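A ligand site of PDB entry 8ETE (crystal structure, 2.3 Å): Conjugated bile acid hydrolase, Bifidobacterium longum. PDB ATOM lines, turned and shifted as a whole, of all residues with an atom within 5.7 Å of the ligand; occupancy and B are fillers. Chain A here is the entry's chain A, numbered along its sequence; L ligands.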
ATOM      1  N   CYS A   2     -13.462   8.771  -9.546  1.00  0.00           N
ATOM      2  CA  CYS A   2     -14.481   9.736  -9.193  1.00  0.00           C
ATOM      3  C   CYS A   2     -14.141  10.473  -7.907  1.00  0.00           C
ATOM      4  O   CYS A   2     -13.204  10.112  -7.206  1.00  0.00           O
ATOM      5  CB  CYS A   2     -15.853   9.075  -9.032  1.00  0.00           C
ATOM      6  SG  CYS A   2     -16.395   8.015 -10.368  1.00  0.00           S
ATOM      7  N   THR A   3     -14.948  11.477  -7.602  1.00  0.00           N
ATOM      8  CA  THR A   3     -14.698  12.377  -6.490  1.00  0.00           C
ATOM      9  C   THR A   3     -16.012  12.668  -5.775  1.00  0.00           C
ATOM     10  O   THR A   3     -17.045  12.861  -6.411  1.00  0.00           O
ATOM     11  CB  THR A   3     -14.079  13.687  -6.974  1.00  0.00           C
ATOM     12  OG1 THR A   3     -12.945  13.416  -7.805  1.00  0.00           O
ATOM     13  CG2 THR A   3     -13.658  14.542  -5.792  1.00  0.00           C
ATOM     14  N   ARG A  18     -20.971  14.698  -6.735  1.00  0.00           N
ATOM     15  CA  ARG A  18     -19.988  13.707  -7.154  1.00  0.00           C
ATOM     16  C   ARG A  18     -19.714  13.856  -8.649  1.00  0.00           C
ATOM     17  O   ARG A  18     -20.569  14.295  -9.415  1.00  0.00           O
ATOM     18  CB  ARG A  18     -20.444  12.277  -6.839  1.00  0.00           C
ATOM     19  CG  ARG A  18     -21.680  11.823  -7.604  1.00  0.00           C
ATOM     20  CD  ARG A  18     -21.319  11.009  -8.851  1.00  0.00           C
ATOM     21  NE  ARG A  18     -20.274  10.014  -8.609  1.00  0.00           N
ATOM     22  CZ  ARG A  18     -20.497   8.799  -8.133  1.00  0.00           C
ATOM     23  NH1 ARG A  18     -21.709   8.388  -7.813  1.00  0.00           N
ATOM     24  NH2 ARG A  18     -19.463   7.966  -7.968  1.00  0.00           N
ATOM     25  N   ASN A  19     -18.510  13.469  -9.034  1.00  0.00           N
ATOM     26  CA  ASN A  19     -18.163  13.214 -10.419  1.00  0.00           C
ATOM     27  C   ASN A  19     -18.268  11.721 -10.665  1.00  0.00           C
ATOM     28  O   ASN A  19     -18.192  10.910  -9.736  1.00  0.00           O
ATOM     29  CB  ASN A  19     -16.751  13.693 -10.747  1.00  0.00           C
ATOM     30  CG  ASN A  19     -16.654  15.204 -10.885  1.00  0.00           C
ATOM     31  OD1 ASN A  19     -17.655  15.887 -11.124  1.00  0.00           O
ATOM     32  ND2 ASN A  19     -15.453  15.735 -10.719  1.00  0.00           N
ATOM     33  N   LEU A  20     -18.444  11.348 -11.928  1.00  0.00           N
ATOM     34  CA  LEU A  20     -18.405   9.938 -12.318  1.00  0.00           C
ATOM     35  C   LEU A  20     -17.449   9.813 -13.500  1.00  0.00           C
ATOM     36  O   LEU A  20     -17.789  10.206 -14.622  1.00  0.00           O
ATOM     37  CB  LEU A  20     -19.795   9.421 -12.666  1.00  0.00           C
ATOM     38  CG  LEU A  20     -19.812   7.968 -13.148  1.00  0.00           C
ATOM     39  CD1 LEU A  20     -20.866   7.189 -12.390  1.00  0.00           C
ATOM     40  CD2 LEU A  20     -20.065   7.892 -14.642  1.00  0.00           C
ATOM     41  N   ASP A  21     -16.275   9.252 -13.243  1.00  0.00           N
ATOM     42  CA  ASP A  21     -15.226   9.097 -14.256  1.00  0.00           C
ATOM     43  C   ASP A  21     -15.242   7.657 -14.764  1.00  0.00           C
ATOM     44  O   ASP A  21     -15.030   6.714 -13.996  1.00  0.00           O
ATOM     45  CB  ASP A  21     -13.848   9.449 -13.692  1.00  0.00           C
ATOM     46  CG  ASP A  21     -13.858  10.733 -12.866  1.00  0.00           C
ATOM     47  OD1 ASP A  21     -14.813  11.538 -12.992  1.00  0.00           O
ATOM     48  OD2 ASP A  21     -12.885  10.950 -12.091  1.00  0.00           O
ATOM     49  N   TRP A  22     -15.478   7.502 -16.067  1.00  0.00           N
ATOM     50  CA  TRP A  22     -15.525   6.184 -16.713  1.00  0.00           C
ATOM     51  C   TRP A  22     -15.421   6.405 -18.219  1.00  0.00           C
ATOM     52  O   TRP A  22     -15.325   7.537 -18.704  1.00  0.00           O
ATOM     53  CB  TRP A  22     -16.780   5.412 -16.315  1.00  0.00           C
ATOM     54  CG  TRP A  22     -16.633   3.924 -16.373  1.00  0.00           C
ATOM     55  CD1 TRP A  22     -17.361   3.054 -17.136  1.00  0.00           C
ATOM     56  CD2 TRP A  22     -15.698   3.116 -15.643  1.00  0.00           C
ATOM     57  NE1 TRP A  22     -16.943   1.766 -16.928  1.00  0.00           N
ATOM     58  CE2 TRP A  22     -15.923   1.776 -16.013  1.00  0.00           C
ATOM     59  CE3 TRP A  22     -14.691   3.397 -14.714  1.00  0.00           C
ATOM     60  CZ2 TRP A  22     -15.182   0.719 -15.490  1.00  0.00           C
ATOM     61  CZ3 TRP A  22     -13.956   2.344 -14.197  1.00  0.00           C
ATOM     62  CH2 TRP A  22     -14.203   1.017 -14.583  1.00  0.00           C
ATOM     63  N   TYR A  26     -23.537   4.160 -18.471  1.00  0.00           N
ATOM     64  CA  TYR A  26     -24.370   3.047 -18.043  1.00  0.00           C
ATOM     65  C   TYR A  26     -25.855   3.320 -18.249  1.00  0.00           C
ATOM     66  O   TYR A  26     -26.690   2.635 -17.635  1.00  0.00           O
ATOM     67  CB  TYR A  26     -24.100   2.716 -16.571  1.00  0.00           C
ATOM     68  CG  TYR A  26     -22.913   1.807 -16.337  1.00  0.00           C
ATOM     69  CD1 TYR A  26     -23.073   0.425 -16.306  1.00  0.00           C
ATOM     70  CD2 TYR A  26     -21.643   2.320 -16.129  1.00  0.00           C
ATOM     71  CE1 TYR A  26     -21.993  -0.411 -16.075  1.00  0.00           C
ATOM     72  CE2 TYR A  26     -20.563   1.494 -15.908  1.00  0.00           C
ATOM     73  CZ  TYR A  26     -20.738   0.129 -15.881  1.00  0.00           C
ATOM     74  OH  TYR A  26     -19.664  -0.710 -15.662  1.00  0.00           O
ATOM     75  N   VAL A  59     -30.055   3.730 -12.573  1.00  0.00           N
ATOM     76  CA  VAL A  59     -30.665   2.867 -13.564  1.00  0.00           C
ATOM     77  C   VAL A  59     -31.744   2.030 -12.894  1.00  0.00           C
ATOM     78  O   VAL A  59     -31.830   1.946 -11.673  1.00  0.00           O
ATOM     79  CB  VAL A  59     -29.622   1.966 -14.286  1.00  0.00           C
ATOM     80  CG1 VAL A  59     -28.505   2.808 -14.871  1.00  0.00           C
ATOM     81  CG2 VAL A  59     -29.071   0.923 -13.328  1.00  0.00           C
ATOM     82  N   MET A  61     -32.605  -1.529 -13.021  1.00  0.00           N
ATOM     83  CA  MET A  61     -32.459  -2.961 -13.274  1.00  0.00           C
ATOM     84  C   MET A  61     -33.521  -3.746 -12.512  1.00  0.00           C
ATOM     85  O   MET A  61     -33.860  -3.412 -11.372  1.00  0.00           O
ATOM     86  CB  MET A  61     -31.060  -3.422 -12.884  1.00  0.00           C
ATOM     87  CG  MET A  61     -30.007  -3.195 -13.961  1.00  0.00           C
ATOM     88  SD  MET A  61     -28.381  -3.834 -13.517  1.00  0.00           S
ATOM     89  CE  MET A  61     -27.357  -3.094 -14.788  1.00  0.00           C
ATOM     90  N   MET A  66     -31.257   1.236  -8.719  1.00  0.00           N
ATOM     91  CA  MET A  66     -29.821   1.089  -8.474  1.00  0.00           C
ATOM     92  C   MET A  66     -29.195   2.478  -8.584  1.00  0.00           C
ATOM     93  O   MET A  66     -28.744   2.900  -9.645  1.00  0.00           O
ATOM     94  CB  MET A  66     -29.183   0.108  -9.446  1.00  0.00           C
ATOM     95  CG  MET A  66     -30.115  -0.996  -9.884  1.00  0.00           C
ATOM     96  SD  MET A  66     -29.915  -2.455  -8.854  1.00  0.00           S
ATOM     97  CE  MET A  66     -28.891  -3.466  -9.921  1.00  0.00           C
ATOM     98  N   TYR A  67     -29.170   3.186  -7.459  1.00  0.00           N
ATOM     99  CA  TYR A  67     -28.685   4.556  -7.431  1.00  0.00           C
ATOM    100  C   TYR A  67     -27.160   4.600  -7.429  1.00  0.00           C
ATOM    101  O   TYR A  67     -26.521   3.924  -6.605  1.00  0.00           O
ATOM    102  CB  TYR A  67     -29.223   5.288  -6.201  1.00  0.00           C
ATOM    103  CG  TYR A  67     -30.598   5.892  -6.376  1.00  0.00           C
ATOM    104  CD1 TYR A  67     -30.782   7.019  -7.180  1.00  0.00           C
ATOM    105  CD2 TYR A  67     -31.706   5.373  -5.726  1.00  0.00           C
ATOM    106  CE1 TYR A  67     -32.041   7.582  -7.340  1.00  0.00           C
ATOM    107  CE2 TYR A  67     -32.964   5.926  -5.876  1.00  0.00           C
ATOM    108  CZ  TYR A  67     -33.125   7.036  -6.688  1.00  0.00           C
ATOM    109  OH  TYR A  67     -34.369   7.591  -6.837  1.00  0.00           O
ATOM    110  N   PHE A  68     -26.584   5.357  -8.363  1.00  0.00           N
ATOM    111  CA  PHE A  68     -25.172   5.718  -8.266  1.00  0.00           C
ATOM    112  C   PHE A  68     -24.945   6.702  -7.128  1.00  0.00           C
ATOM    113  O   PHE A  68     -23.969   6.593  -6.384  1.00  0.00           O
ATOM    114  CB  PHE A  68     -24.665   6.315  -9.574  1.00  0.00           C
ATOM    115  CG  PHE A  68     -25.130   5.598 -10.826  1.00  0.00           C
ATOM    116  CD1 PHE A  68     -24.242   4.841 -11.558  1.00  0.00           C
ATOM    117  CD2 PHE A  68     -26.417   5.749 -11.305  1.00  0.00           C
ATOM    118  CE1 PHE A  68     -24.641   4.192 -12.711  1.00  0.00           C
ATOM    119  CE2 PHE A  68     -26.823   5.104 -12.464  1.00  0.00           C
ATOM    120  CZ  PHE A  68     -25.936   4.334 -13.169  1.00  0.00           C
ATOM    121  N   GLY A  80     -21.579   6.185  -4.185  1.00  0.00           N
ATOM    122  CA  GLY A  80     -20.675   5.032  -4.220  1.00  0.00           C
ATOM    123  C   GLY A  80     -19.587   5.235  -5.253  1.00  0.00           C
ATOM    124  O   GLY A  80     -19.827   5.766  -6.340  1.00  0.00           O
ATOM    125  N   LEU A  81     -18.373   4.804  -4.905  1.00  0.00           N
ATOM    126  CA  LEU A  81     -17.189   4.991  -5.726  1.00  0.00           C
ATOM    127  C   LEU A  81     -16.403   3.691  -5.817  1.00  0.00           C
ATOM    128  O   LEU A  81     -16.379   2.901  -4.875  1.00  0.00           O
ATOM    129  CB  LEU A  81     -16.286   6.117  -5.174  1.00  0.00           C
ATOM    130  CG  LEU A  81     -16.874   7.533  -5.124  1.00  0.00           C
ATOM    131  CD1 LEU A  81     -17.567   7.792  -3.794  1.00  0.00           C
ATOM    132  CD2 LEU A  81     -15.775   8.561  -5.345  1.00  0.00           C
ATOM    133  N   ASN A  82     -15.728   3.503  -6.951  1.00  0.00           N
ATOM    134  CA  ASN A  82     -15.001   2.267  -7.226  1.00  0.00           C
ATOM    135  C   ASN A  82     -13.890   2.055  -6.208  1.00  0.00           C
ATOM    136  O   ASN A  82     -13.107   2.962  -5.936  1.00  0.00           O
ATOM    137  CB  ASN A  82     -14.446   2.328  -8.649  1.00  0.00           C
ATOM    138  CG  ASN A  82     -14.403   0.986  -9.343  1.00  0.00           C
ATOM    139  OD1 ASN A  82     -13.334   0.464  -9.659  1.00  0.00           O
ATOM    140  ND2 ASN A  82     -15.566   0.382  -9.545  1.00  0.00           N
ATOM    141  N   THR A 102     -25.281  -4.944  -1.680  1.00  0.00           N
ATOM    142  CA  THR A 102     -24.468  -3.793  -2.049  1.00  0.00           C
ATOM    143  C   THR A 102     -25.259  -2.822  -2.931  1.00  0.00           C
ATOM    144  O   THR A 102     -25.242  -1.613  -2.688  1.00  0.00           O
ATOM    145  CB  THR A 102     -23.195  -4.253  -2.774  1.00  0.00           C
ATOM    146  OG1 THR A 102     -23.528  -4.865  -4.024  1.00  0.00           O
ATOM    147  CG2 THR A 102     -22.416  -5.239  -1.908  1.00  0.00           C
ATOM    148  N   PHE A 103     -25.963  -3.337  -3.938  1.00  0.00           N
ATOM    149  CA  PHE A 103     -26.655  -2.469  -4.887  1.00  0.00           C
ATOM    150  C   PHE A 103     -27.821  -1.735  -4.230  1.00  0.00           C
ATOM    151  O   PHE A 103     -28.212  -0.659  -4.705  1.00  0.00           O
ATOM    152  CB  PHE A 103     -27.144  -3.273  -6.085  1.00  0.00           C
ATOM    153  CG  PHE A 103     -27.710  -4.622  -5.725  1.00  0.00           C
ATOM    154  CD1 PHE A 103     -29.061  -4.757  -5.401  1.00  0.00           C
ATOM    155  CD2 PHE A 103     -26.904  -5.749  -5.700  1.00  0.00           C
ATOM    156  CE1 PHE A 103     -29.579  -5.996  -5.071  1.00  0.00           C
ATOM    157  CE2 PHE A 103     -27.422  -6.988  -5.370  1.00  0.00           C
ATOM    158  CZ  PHE A 103     -28.759  -7.111  -5.055  1.00  0.00           C
ATOM    159  N   GLN A 137     -19.234  -9.043 -13.499  1.00  0.00           N
ATOM    160  CA  GLN A 137     -18.351  -8.686 -12.396  1.00  0.00           C
ATOM    161  C   GLN A 137     -19.115  -7.979 -11.274  1.00  0.00           C
ATOM    162  O   GLN A 137     -20.026  -7.181 -11.541  1.00  0.00           O
ATOM    163  CB  GLN A 137     -17.207  -7.804 -12.890  1.00  0.00           C
ATOM    164  N   SER A 139     -19.690  -5.356  -8.144  1.00  0.00           N
ATOM    165  CA  SER A 139     -19.292  -3.985  -7.850  1.00  0.00           C
ATOM    166  C   SER A 139     -18.549  -3.951  -6.507  1.00  0.00           C
ATOM    167  O   SER A 139     -19.101  -4.345  -5.475  1.00  0.00           O
ATOM    168  CB  SER A 139     -20.515  -3.072  -7.826  1.00  0.00           C
ATOM    169  OG  SER A 139     -21.144  -3.092  -6.551  1.00  0.00           O
ATOM    170  N   LEU A 141     -17.137  -1.359  -4.092  1.00  0.00           N
ATOM    171  CA  LEU A 141     -17.269   0.067  -3.845  1.00  0.00           C
ATOM    172  C   LEU A 141     -17.080   0.399  -2.371  1.00  0.00           C
ATOM    173  O   LEU A 141     -17.195  -0.464  -1.490  1.00  0.00           O
ATOM    174  CB  LEU A 141     -18.649   0.596  -4.299  1.00  0.00           C
ATOM    175  CG  LEU A 141     -19.219   0.150  -5.634  1.00  0.00           C
ATOM    176  CD1 LEU A 141     -20.568   0.817  -5.867  1.00  0.00           C
ATOM    177  CD2 LEU A 141     -18.265   0.483  -6.772  1.00  0.00           C
ATOM    178  N   ASN A 173     -11.262   7.331  -4.937  1.00  0.00           N
ATOM    179  CA  ASN A 173     -11.023   5.893  -5.058  1.00  0.00           C
ATOM    180  C   ASN A 173      -9.830   5.384  -4.244  1.00  0.00           C
ATOM    181  O   ASN A 173      -9.536   5.897  -3.155  1.00  0.00           O
ATOM    182  CB  ASN A 173     -10.839   5.523  -6.524  1.00  0.00           C
ATOM    183  CG  ASN A 173     -11.897   6.159  -7.414  1.00  0.00           C
ATOM    184  OD1 ASN A 173     -11.577   6.857  -8.370  1.00  0.00           O
ATOM    185  ND2 ASN A 173     -13.160   5.914  -7.095  1.00  0.00           N
HETATM  186  C1  LIG L   1     -17.842   4.359 -11.260  1.00  0.00           C
HETATM  187  C2  LIG L   1     -25.179  -0.923  -9.869  1.00  0.00           C
HETATM  188  C3  LIG L   1     -18.551   3.102 -11.770  1.00  0.00           C
HETATM  189  C4  LIG L   1     -17.535   2.006 -12.095  1.00  0.00           C
HETATM  190  C5  LIG L   1     -23.126   1.145 -10.386  1.00  0.00           C
HETATM  191  C6  LIG L   1     -19.655   2.649 -10.790  1.00  0.00           C
HETATM  192  C7  LIG L   1     -20.414   3.841 -10.154  1.00  0.00           C
HETATM  193  C8  LIG L   1     -21.786   3.299  -9.689  1.00  0.00           C
HETATM  194  C9  LIG L   1     -21.789   1.831 -10.126  1.00  0.00           C
HETATM  195  C10 LIG L   1     -24.074   1.239  -9.186  1.00  0.00           C
HETATM  196  C11 LIG L   1     -25.400   0.531  -9.479  1.00  0.00           C
HETATM  197  C12 LIG L   1     -16.851   4.138 -10.125  1.00  0.00           C
HETATM  198  C13 LIG L   1     -16.899   6.575  -9.475  1.00  0.00           C
HETATM  199  C14 LIG L   1     -24.739  -1.766  -8.672  1.00  0.00           C
HETATM  200  C15 LIG L   1     -24.528  -3.225  -9.016  1.00  0.00           C
HETATM  201  C16 LIG L   1     -23.545  -3.355 -10.163  1.00  0.00           C
HETATM  202  C17 LIG L   1     -24.009  -2.562 -11.369  1.00  0.00           C
HETATM  203  C18 LIG L   1     -24.226  -1.062 -11.094  1.00  0.00           C
HETATM  204  C19 LIG L   1     -16.096   5.383  -9.780  1.00  0.00           C
HETATM  205  C20 LIG L   1     -24.870  -0.445 -12.353  1.00  0.00           C
HETATM  206  C21 LIG L   1     -22.890  -0.335 -10.762  1.00  0.00           C
HETATM  207  C22 LIG L   1     -21.830  -0.486 -11.862  1.00  0.00           C
HETATM  208  C23 LIG L   1     -20.537   0.288 -11.582  1.00  0.00           C
HETATM  209  C24 LIG L   1     -20.830   1.772 -11.331  1.00  0.00           C
HETATM  210  C25 LIG L   1     -21.437   2.440 -12.578  1.00  0.00           C
HETATM  211  O1  LIG L   1     -14.882   5.411  -9.782  1.00  0.00           O
HETATM  212  O2  LIG L   1     -24.061  -3.944  -7.867  1.00  0.00           O
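O2 of the ligand lies within hydrogen-bond range of OG of Ser 139 (3.3 Å). SG of Cys 2 is bonded to C13 of the ligand (1.8 Å). The side-chain amide nitrogen (ND2) of Asn 173 lies within hydrogen-bond range of an oxygen (O1) of the ligand, 3.2 Å away.
The backbone carbonyl oxygen (O) of Asn 82 sits at hydrogen-bond distance from the side-chain amide nitrogen (ND2) of Asn 173 (3.2 Å). The backbone carbonyl oxygen of Gly 80 lies within hydrogen-bond range of the guanidinium group of Arg 18, 2.8 Å away. The backbone carbonyl oxygen of Val 59 lies within hydrogen-bond range of the backbone NH of Met 66 (3.1 Å). OD1 of Asn 173 sits at hydrogen-bond distance from N of Cys 2, 2.9 Å away. SG of Cys 2 is in hydrogen-bond range of N of Asp 21 (3.1 Å). O of Phe 68 is in hydrogen-bond range of N of Gly 80, 3.3 Å away. The guanidinium group of Arg 18 lies within hydrogen-bond range of the backbone carbonyl oxygen of Phe 68 (3.2 Å).
NH2 of Arg 18 touches C13 of the ligand (3.3 Å). CD2 of Tyr 26 touches C25 of the ligand (3.6 Å). Met 66 touches the ligand (CB to C11, 3.8 Å). CD1 of Phe 68 touches C8 of the ligand, 3.5 Å away. Asn 82 touches the ligand (CB to O1, 3.3 Å). OG1 of Thr 102 touches O2 of the ligand (3.99 Å). CB of Phe 103 touches O2 of the ligand, at 3.6 Å. Hydrophobic or aromatic side chains within 4 Å of the ligand: Tyr 26, Met 66, Phe 68 and Phe 103. Within 4 Å of the ligand: Cys 2, Arg 18, Tyr 26, Met 66, Phe 68, Asn 82, Thr 102, Phe 103, Ser 139 and Asn 173. The nearest printed residue that does not touch the ligand is Leu 20 (4.1 Å).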
